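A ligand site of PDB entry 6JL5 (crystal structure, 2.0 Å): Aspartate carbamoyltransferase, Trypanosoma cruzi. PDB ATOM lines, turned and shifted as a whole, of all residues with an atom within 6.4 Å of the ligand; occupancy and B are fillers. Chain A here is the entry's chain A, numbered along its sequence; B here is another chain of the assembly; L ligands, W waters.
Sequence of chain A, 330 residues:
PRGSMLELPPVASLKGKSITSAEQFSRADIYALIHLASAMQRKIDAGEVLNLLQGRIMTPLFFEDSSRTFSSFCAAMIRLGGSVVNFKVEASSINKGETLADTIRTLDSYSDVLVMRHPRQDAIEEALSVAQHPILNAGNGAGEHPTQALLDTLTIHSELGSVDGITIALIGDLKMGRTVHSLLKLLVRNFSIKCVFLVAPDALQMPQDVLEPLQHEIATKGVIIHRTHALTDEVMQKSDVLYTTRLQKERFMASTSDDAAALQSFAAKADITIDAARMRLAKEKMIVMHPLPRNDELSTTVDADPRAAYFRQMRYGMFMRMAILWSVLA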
ATOM      1  N   GLU A  64       0.957 -39.508   8.557  1.00  0.00           N
ATOM      2  CA  GLU A  64       2.235 -38.819   8.222  1.00  0.00           C
ATOM      3  C   GLU A  64       2.570 -37.829   9.338  1.00  0.00           C
ATOM      4  O   GLU A  64       1.703 -37.395  10.104  1.00  0.00           O
ATOM      5  CB  GLU A  64       2.149 -37.999   6.913  1.00  0.00           C
ATOM      6  CG  GLU A  64       1.855 -38.741   5.614  1.00  0.00           C
ATOM      7  CD  GLU A  64       1.969 -37.838   4.361  1.00  0.00           C
ATOM      8  OE1 GLU A  64       1.513 -36.684   4.375  1.00  0.00           O
ATOM      9  OE2 GLU A  64       2.496 -38.292   3.342  1.00  0.00           O
ATOM     10  N   ASP A  65       3.813 -37.393   9.378  1.00  0.00           N
ATOM     11  CA  ASP A  65       4.258 -36.386  10.322  1.00  0.00           C
ATOM     12  C   ASP A  65       3.643 -35.012  10.038  1.00  0.00           C
ATOM     13  O   ASP A  65       3.404 -34.668   8.894  1.00  0.00           O
ATOM     14  CB  ASP A  65       5.779 -36.279  10.256  1.00  0.00           C
ATOM     15  CG  ASP A  65       6.473 -37.427  10.976  1.00  0.00           C
ATOM     16  OD1 ASP A  65       5.807 -38.193  11.719  1.00  0.00           O
ATOM     17  OD2 ASP A  65       7.705 -37.562  10.811  1.00  0.00           O
ATOM     18  N   ARG A  68       2.479 -28.085  11.987  1.00  0.00           N
ATOM     19  CA  ARG A  68       1.396 -27.078  11.886  1.00  0.00           C
ATOM     20  C   ARG A  68      -0.022 -27.644  11.878  1.00  0.00           C
ATOM     21  O   ARG A  68      -0.846 -27.249  12.684  1.00  0.00           O
ATOM     22  CB  ARG A  68       1.552 -26.264  10.586  1.00  0.00           C
ATOM     23  CG  ARG A  68       2.455 -25.088  10.713  1.00  0.00           C
ATOM     24  CD  ARG A  68       3.231 -24.907   9.423  1.00  0.00           C
ATOM     25  NE  ARG A  68       4.079 -26.071   9.243  1.00  0.00           N
ATOM     26  CZ  ARG A  68       5.295 -26.190   9.762  1.00  0.00           C
ATOM     27  NH1 ARG A  68       5.845 -25.188  10.430  1.00  0.00           N
ATOM     28  NH2 ARG A  68       5.940 -27.322   9.595  1.00  0.00           N
ATOM     29  N   THR A  69      -0.312 -28.504  10.917  1.00  0.00           N
ATOM     30  CA  THR A  69      -1.656 -28.959  10.684  1.00  0.00           C
ATOM     31  C   THR A  69      -2.182 -29.747  11.899  1.00  0.00           C
ATOM     32  O   THR A  69      -3.255 -29.422  12.367  1.00  0.00           O
ATOM     33  CB  THR A  69      -1.751 -29.766   9.364  1.00  0.00           C
ATOM     34  OG1 THR A  69      -1.173 -28.959   8.317  1.00  0.00           O
ATOM     35  CG2 THR A  69      -3.217 -30.048   9.014  1.00  0.00           C
ATOM     36  N   ARG A 117      -4.765 -37.186   7.899  1.00  0.00           N
ATOM     37  CA  ARG A 117      -3.644 -37.016   6.965  1.00  0.00           C
ATOM     38  C   ARG A 117      -3.064 -38.391   6.619  1.00  0.00           C
ATOM     39  O   ARG A 117      -2.794 -39.199   7.520  1.00  0.00           O
ATOM     40  CB  ARG A 117      -2.553 -36.116   7.529  1.00  0.00           C
ATOM     41  CG  ARG A 117      -1.251 -36.112   6.701  1.00  0.00           C
ATOM     42  CD  ARG A 117      -0.210 -35.074   7.184  1.00  0.00           C
ATOM     43  NE  ARG A 117      -0.611 -33.750   6.763  1.00  0.00           N
ATOM     44  CZ  ARG A 117       0.130 -32.641   6.845  1.00  0.00           C
ATOM     45  NH1 ARG A 117       1.358 -32.652   7.381  1.00  0.00           N
ATOM     46  NH2 ARG A 117      -0.385 -31.510   6.383  1.00  0.00           N
ATOM     47  N   ALA A 138      -6.609 -33.288   5.993  1.00  0.00           N
ATOM     48  CA  ALA A 138      -5.398 -32.571   6.419  1.00  0.00           C
ATOM     49  C   ALA A 138      -4.187 -32.882   5.477  1.00  0.00           C
ATOM     50  O   ALA A 138      -3.045 -32.534   5.779  1.00  0.00           O
ATOM     51  CB  ALA A 138      -5.062 -32.928   7.871  1.00  0.00           C
ATOM     52  N   GLY A 139      -4.452 -33.501   4.322  1.00  0.00           N
ATOM     53  CA  GLY A 139      -3.410 -33.769   3.306  1.00  0.00           C
ATOM     54  C   GLY A 139      -3.464 -35.199   2.794  1.00  0.00           C
ATOM     55  O   GLY A 139      -3.326 -36.148   3.572  1.00  0.00           O
ATOM     56  N   GLY A 141      -1.677 -37.577   0.240  1.00  0.00           N
ATOM     57  CA  GLY A 141      -0.585 -37.824  -0.713  1.00  0.00           C
ATOM     58  C   GLY A 141      -0.178 -36.502  -1.334  1.00  0.00           C
ATOM     59  O   GLY A 141      -0.047 -35.470  -0.618  1.00  0.00           O
ATOM     60  N   HIS A 145      -4.655 -30.167   0.041  1.00  0.00           N
ATOM     61  CA  HIS A 145      -4.615 -29.713   1.439  1.00  0.00           C
ATOM     62  C   HIS A 145      -5.618 -28.533   1.472  1.00  0.00           C
ATOM     63  O   HIS A 145      -5.217 -27.376   1.468  1.00  0.00           O
ATOM     64  CB  HIS A 145      -3.201 -29.242   1.748  1.00  0.00           C
ATOM     65  CG  HIS A 145      -2.855 -29.168   3.216  1.00  0.00           C
ATOM     66  ND1 HIS A 145      -3.798 -28.978   4.209  1.00  0.00           N
ATOM     67  CD2 HIS A 145      -1.652 -29.188   3.828  1.00  0.00           C
ATOM     68  CE1 HIS A 145      -3.179 -28.941   5.383  1.00  0.00           C
ATOM     69  NE2 HIS A 145      -1.878 -29.062   5.172  1.00  0.00           N
ATOM     70  N   GLN A 148      -5.351 -25.718   4.128  1.00  0.00           N
ATOM     71  CA  GLN A 148      -4.197 -24.844   3.901  1.00  0.00           C
ATOM     72  C   GLN A 148      -4.565 -23.777   2.864  1.00  0.00           C
ATOM     73  O   GLN A 148      -4.226 -22.595   3.029  1.00  0.00           O
ATOM     74  CB  GLN A 148      -2.984 -25.651   3.432  1.00  0.00           C
ATOM     75  CG  GLN A 148      -1.712 -24.786   3.234  1.00  0.00           C
ATOM     76  CD  GLN A 148      -1.032 -24.435   4.560  1.00  0.00           C
ATOM     77  OE1 GLN A 148      -0.839 -25.311   5.431  1.00  0.00           O
ATOM     78  NE2 GLN A 148      -0.640 -23.178   4.713  1.00  0.00           N
ATOM     79  N   MET A 176       4.523 -32.227  -6.671  1.00  0.00           N
ATOM     80  CA  MET A 176       4.149 -32.998  -5.471  1.00  0.00           C
ATOM     81  C   MET A 176       3.504 -32.144  -4.372  1.00  0.00           C
ATOM     82  O   MET A 176       3.025 -32.691  -3.363  1.00  0.00           O
ATOM     83  CB  MET A 176       5.347 -33.758  -4.887  1.00  0.00           C
ATOM     84  CG  MET A 176       6.102 -34.622  -5.946  1.00  0.00           C
ATOM     85  SD  MET A 176       5.007 -35.828  -6.779  1.00  0.00           S
ATOM     86  CE  MET A 176       5.078 -37.175  -5.628  1.00  0.00           C
ATOM     87  N   GLY A 177       3.457 -30.823  -4.578  1.00  0.00           N
ATOM     88  CA  GLY A 177       2.973 -29.910  -3.551  1.00  0.00           C
ATOM     89  C   GLY A 177       1.460 -29.827  -3.483  1.00  0.00           C
ATOM     90  O   GLY A 177       0.838 -29.106  -4.275  1.00  0.00           O
ATOM     91  N   ARG A 178       0.873 -30.573  -2.536  1.00  0.00           N
ATOM     92  CA  ARG A 178      -0.576 -30.573  -2.353  1.00  0.00           C
ATOM     93  C   ARG A 178      -1.094 -29.189  -1.954  1.00  0.00           C
ATOM     94  O   ARG A 178      -2.235 -28.850  -2.256  1.00  0.00           O
ATOM     95  CB  ARG A 178      -1.026 -31.613  -1.317  1.00  0.00           C
ATOM     96  CG  ARG A 178      -0.369 -31.479   0.080  1.00  0.00           C
ATOM     97  CD  ARG A 178      -0.669 -32.714   0.910  1.00  0.00           C
ATOM     98  NE  ARG A 178       0.122 -32.725   2.123  1.00  0.00           N
ATOM     99  CZ  ARG A 178       0.423 -33.825   2.807  1.00  0.00           C
ATOM    100  NH1 ARG A 178       1.167 -33.728   3.920  1.00  0.00           N
ATOM    101  NH2 ARG A 178      -0.012 -35.018   2.384  1.00  0.00           N
ATOM    102  N   THR A 179      -0.258 -28.363  -1.308  1.00  0.00           N
ATOM    103  CA  THR A 179      -0.698 -27.006  -0.956  1.00  0.00           C
ATOM    104  C   THR A 179      -0.950 -26.126  -2.212  1.00  0.00           C
ATOM    105  O   THR A 179      -1.966 -25.436  -2.294  1.00  0.00           O
ATOM    106  CB  THR A 179       0.296 -26.340  -0.020  1.00  0.00           C
ATOM    107  OG1 THR A 179       1.543 -26.209  -0.702  1.00  0.00           O
ATOM    108  CG2 THR A 179       0.502 -27.192   1.244  1.00  0.00           C
ATOM    109  N   THR A 245       7.633 -23.143  -1.784  1.00  0.00           N
ATOM    110  CA  THR A 245       7.477 -24.465  -1.207  1.00  0.00           C
ATOM    111  C   THR A 245       8.814 -25.224  -1.160  1.00  0.00           C
ATOM    112  O   THR A 245       9.752 -24.885  -1.846  1.00  0.00           O
ATOM    113  CB  THR A 245       6.502 -25.333  -2.033  1.00  0.00           C
ATOM    114  OG1 THR A 245       7.024 -25.480  -3.359  1.00  0.00           O
ATOM    115  CG2 THR A 245       5.074 -24.726  -2.073  1.00  0.00           C
ATOM    116  N   ARG A 246       8.847 -26.250  -0.336  1.00  0.00           N
ATOM    117  CA  ARG A 246      10.009 -27.097  -0.145  1.00  0.00           C
ATOM    118  C   ARG A 246       9.978 -28.164  -1.231  1.00  0.00           C
ATOM    119  O   ARG A 246       8.892 -28.657  -1.579  1.00  0.00           O
ATOM    120  CB  ARG A 246       9.854 -27.762   1.231  1.00  0.00           C
ATOM    121  CG  ARG A 246      11.002 -28.626   1.702  1.00  0.00           C
ATOM    122  CD  ARG A 246      10.719 -29.230   3.079  1.00  0.00           C
ATOM    123  NE  ARG A 246       9.415 -29.888   3.126  1.00  0.00           N
ATOM    124  CZ  ARG A 246       9.188 -31.183   2.855  1.00  0.00           C
ATOM    125  NH1 ARG A 246      10.196 -31.993   2.496  1.00  0.00           N
ATOM    126  NH2 ARG A 246       7.941 -31.659   2.935  1.00  0.00           N
ATOM    127  N   GLN A 248       9.878 -31.652  -2.109  1.00  0.00           N
ATOM    128  CA  GLN A 248       9.289 -32.681  -1.254  1.00  0.00           C
ATOM    129  C   GLN A 248      10.171 -33.911  -0.972  1.00  0.00           C
ATOM    130  O   GLN A 248      10.919 -34.402  -1.793  1.00  0.00           O
ATOM    131  CB  GLN A 248       7.920 -33.094  -1.748  1.00  0.00           C
ATOM    132  CG  GLN A 248       6.913 -31.963  -1.907  1.00  0.00           C
ATOM    133  CD  GLN A 248       6.488 -31.321  -0.597  1.00  0.00           C
ATOM    134  OE1 GLN A 248       5.859 -31.938   0.229  1.00  0.00           O
ATOM    135  NE2 GLN A 248       6.833 -30.089  -0.420  1.00  0.00           N
ATOM    136  N   HIS A 290       4.825 -19.189   2.670  1.00  0.00           N
ATOM    137  CA  HIS A 290       5.352 -20.544   2.594  1.00  0.00           C
ATOM    138  C   HIS A 290       4.462 -21.382   3.517  1.00  0.00           C
ATOM    139  O   HIS A 290       4.327 -21.045   4.690  1.00  0.00           O
ATOM    140  CB  HIS A 290       6.835 -20.540   3.073  1.00  0.00           C
ATOM    141  CG  HIS A 290       7.597 -21.777   2.719  1.00  0.00           C
ATOM    142  ND1 HIS A 290       7.074 -23.040   2.899  1.00  0.00           N
ATOM    143  CD2 HIS A 290       8.833 -21.955   2.204  1.00  0.00           C
ATOM    144  CE1 HIS A 290       7.952 -23.942   2.488  1.00  0.00           C
ATOM    145  NE2 HIS A 290       9.035 -23.307   2.070  1.00  0.00           N
ATOM    146  N   PRO A 291       3.851 -22.475   3.007  1.00  0.00           N
ATOM    147  CA  PRO A 291       3.008 -23.266   3.962  1.00  0.00           C
ATOM    148  C   PRO A 291       3.835 -23.937   5.075  1.00  0.00           C
ATOM    149  O   PRO A 291       3.267 -24.336   6.083  1.00  0.00           O
ATOM    150  CB  PRO A 291       2.396 -24.347   3.055  1.00  0.00           C
ATOM    151  CG  PRO A 291       3.497 -24.579   1.938  1.00  0.00           C
ATOM    152  CD  PRO A 291       4.035 -23.155   1.700  1.00  0.00           C
ATOM    153  N   LEU A 292       5.156 -24.074   4.850  1.00  0.00           N
ATOM    154  CA  LEU A 292       6.143 -24.669   5.791  1.00  0.00           C
ATOM    155  C   LEU A 292       5.912 -26.184   5.940  1.00  0.00           C
ATOM    156  O   LEU A 292       4.797 -26.649   5.663  1.00  0.00           O
ATOM    157  CB  LEU A 292       6.134 -23.929   7.168  1.00  0.00           C
ATOM    158  CG  LEU A 292       6.429 -22.415   7.167  1.00  0.00           C
ATOM    159  CD1 LEU A 292       6.423 -21.806   8.611  1.00  0.00           C
ATOM    160  CD2 LEU A 292       7.757 -22.139   6.513  1.00  0.00           C
ATOM    161  N   PRO A 293       6.953 -26.945   6.356  1.00  0.00           N
ATOM    162  CA  PRO A 293       8.303 -26.489   6.757  1.00  0.00           C
ATOM    163  C   PRO A 293       9.121 -26.048   5.556  1.00  0.00           C
ATOM    164  O   PRO A 293       8.881 -26.512   4.443  1.00  0.00           O
ATOM    165  CB  PRO A 293       8.925 -27.721   7.414  1.00  0.00           C
ATOM    166  CG  PRO A 293       8.295 -28.892   6.645  1.00  0.00           C
ATOM    167  CD  PRO A 293       6.831 -28.428   6.394  1.00  0.00           C
ATOM    168  N   ARG A 294      10.032 -25.119   5.786  1.00  0.00           N
ATOM    169  CA  ARG A 294      10.990 -24.678   4.793  1.00  0.00           C
ATOM    170  C   ARG A 294      12.322 -25.371   4.960  1.00  0.00           C
ATOM    171  O   ARG A 294      12.674 -25.797   6.048  1.00  0.00           O
ATOM    172  CB  ARG A 294      11.205 -23.152   4.852  1.00  0.00           C
ATOM    173  CG  ARG A 294      11.671 -22.679   6.198  1.00  0.00           C
ATOM    174  CD  ARG A 294      12.273 -21.308   6.125  1.00  0.00           C
ATOM    175  NE  ARG A 294      12.454 -20.779   7.467  1.00  0.00           N
ATOM    176  CZ  ARG A 294      12.885 -19.560   7.736  1.00  0.00           C
ATOM    177  NH1 ARG A 294      13.221 -18.734   6.726  1.00  0.00           N
ATOM    178  NH2 ARG A 294      12.940 -19.155   9.006  1.00  0.00           N
ATOM    179  N   SER B  93       7.358 -32.148  11.862  1.00  0.00           N
ATOM    180  CA  SER B  93       8.047 -31.718  10.641  1.00  0.00           C
ATOM    181  C   SER B  93       9.587 -31.488  10.824  1.00  0.00           C
ATOM    182  O   SER B  93      10.305 -31.247   9.833  1.00  0.00           O
ATOM    183  CB  SER B  93       7.311 -30.563   9.936  1.00  0.00           C
ATOM    184  OG  SER B  93       6.046 -31.004   9.431  1.00  0.00           O
ATOM    185  N   LYS B  96      11.209 -33.464   8.266  1.00  0.00           N
ATOM    186  CA  LYS B  96      11.374 -32.947   6.907  1.00  0.00           C
ATOM    187  C   LYS B  96      12.460 -31.841   6.914  1.00  0.00           C
ATOM    188  O   LYS B  96      12.476 -30.945   6.060  1.00  0.00           O
ATOM    189  CB  LYS B  96      10.028 -32.371   6.409  1.00  0.00           C
ATOM    190  CG  LYS B  96       8.816 -33.335   6.417  1.00  0.00           C
ATOM    191  CD  LYS B  96       7.480 -32.530   6.480  1.00  0.00           C
ATOM    192  CE  LYS B  96       6.242 -33.319   5.997  1.00  0.00           C
ATOM    193  NZ  LYS B  96       5.083 -32.388   5.797  1.00  0.00           N
HETATM  194  N1  LIG L   1       3.437 -28.846   5.257  1.00  0.00           N
HETATM  195  C1  LIG L   1       2.910 -28.857   3.857  1.00  0.00           C
HETATM  196  C2  LIG L   1       2.223 -30.195   3.558  1.00  0.00           C
HETATM  197  O1  LIG L   1       2.087 -31.006   4.440  1.00  0.00           O
HETATM  198  C3  LIG L   1       4.024 -28.546   2.837  1.00  0.00           C
HETATM  199  C4  LIG L   1       5.308 -29.384   3.060  1.00  0.00           C
HETATM  200  O2  LIG L   1       6.393 -28.901   2.654  1.00  0.00           O
HETATM  201  O3  LIG L   1       5.250 -30.486   3.645  1.00  0.00           O
HETATM  202  O4  LIG L   1       1.798 -30.534   2.459  1.00  0.00           O
HETATM  203  O   HOH W   1       1.234 -27.012   5.846  1.00  0.00           O
HETATM  204  O   HOH W   2       2.948 -30.228   0.046  1.00  0.00           O
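NE of Arg 178 lies within salt-bridge range of O4 of the ligand, at 2.8 Å. An oxygen (O3) of the ligand lies within salt-bridge range of the side-chain amino group (NZ) of Lys 96 of chain B. The guanidinium group (NH2) of Arg 117 lies within salt-bridge range of an oxygen (O1) of the ligand (3.2 Å). The backbone carbonyl oxygen (O) of Leu 292 is in hydrogen-bond range of a nitrogen (N1) of the ligand (2.6 Å). The guanidinium group (NH2) of Arg 246 lies within salt-bridge range of an oxygen (O3) of the ligand (3.0 Å). The side-chain amide nitrogen (NE2) of Gln 248 lies within hydrogen-bond range of an oxygen (O2) of the ligand (3.3 Å).
NE2 of His 145 sits at hydrogen-bond distance from OG1 of Thr 69, at 3.2 Å. N of Leu 292 is in hydrogen-bond range of ND1 of His 290. The backbone carbonyl oxygen of Gly 141 is in hydrogen-bond range of the guanidinium group of Arg 178. NH2 of Arg 117 lies within hydrogen-bond range of NE2 of His 145 (3.1 Å). The backbone carbonyl oxygen (O) of Arg 246 lies within hydrogen-bond range of the side-chain amide nitrogen (NE2) of Gln 248. NH1 of Arg 117 lies within hydrogen-bond range of O of Asp 65. The guanidinium group (NE) of Arg 117 lies within hydrogen-bond range of the backbone carbonyl oxygen (O) of Ala 138 (2.9 Å). OE1 of Glu 64 is in salt-bridge range of NH1 of Arg 178, at 3.0 Å.
His 145 touches the ligand. Thr 179 touches the ligand (CG2 to O4, 3.8 Å). CD of Pro 293 touches N1 of the ligand (3.6 Å). Nine residues have an atom within 4 Å of the ligand: Arg 117, His 145, Arg 178, Thr 179, Arg 246, Gln 248, Leu 292, Pro 293 and Lys 96 of chain B.
Water W2 lies within hydrogen-bond range of an oxygen (O4) of the ligand, the backbone NH of Arg 178 and the side-chain amide oxygen of Gln 248. Water W1 lies within hydrogen-bond range of OE1 of Gln 148 (2.7 Å), N1 of the ligand (2.9 Å) and O of Pro 291 (3.4 Å).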
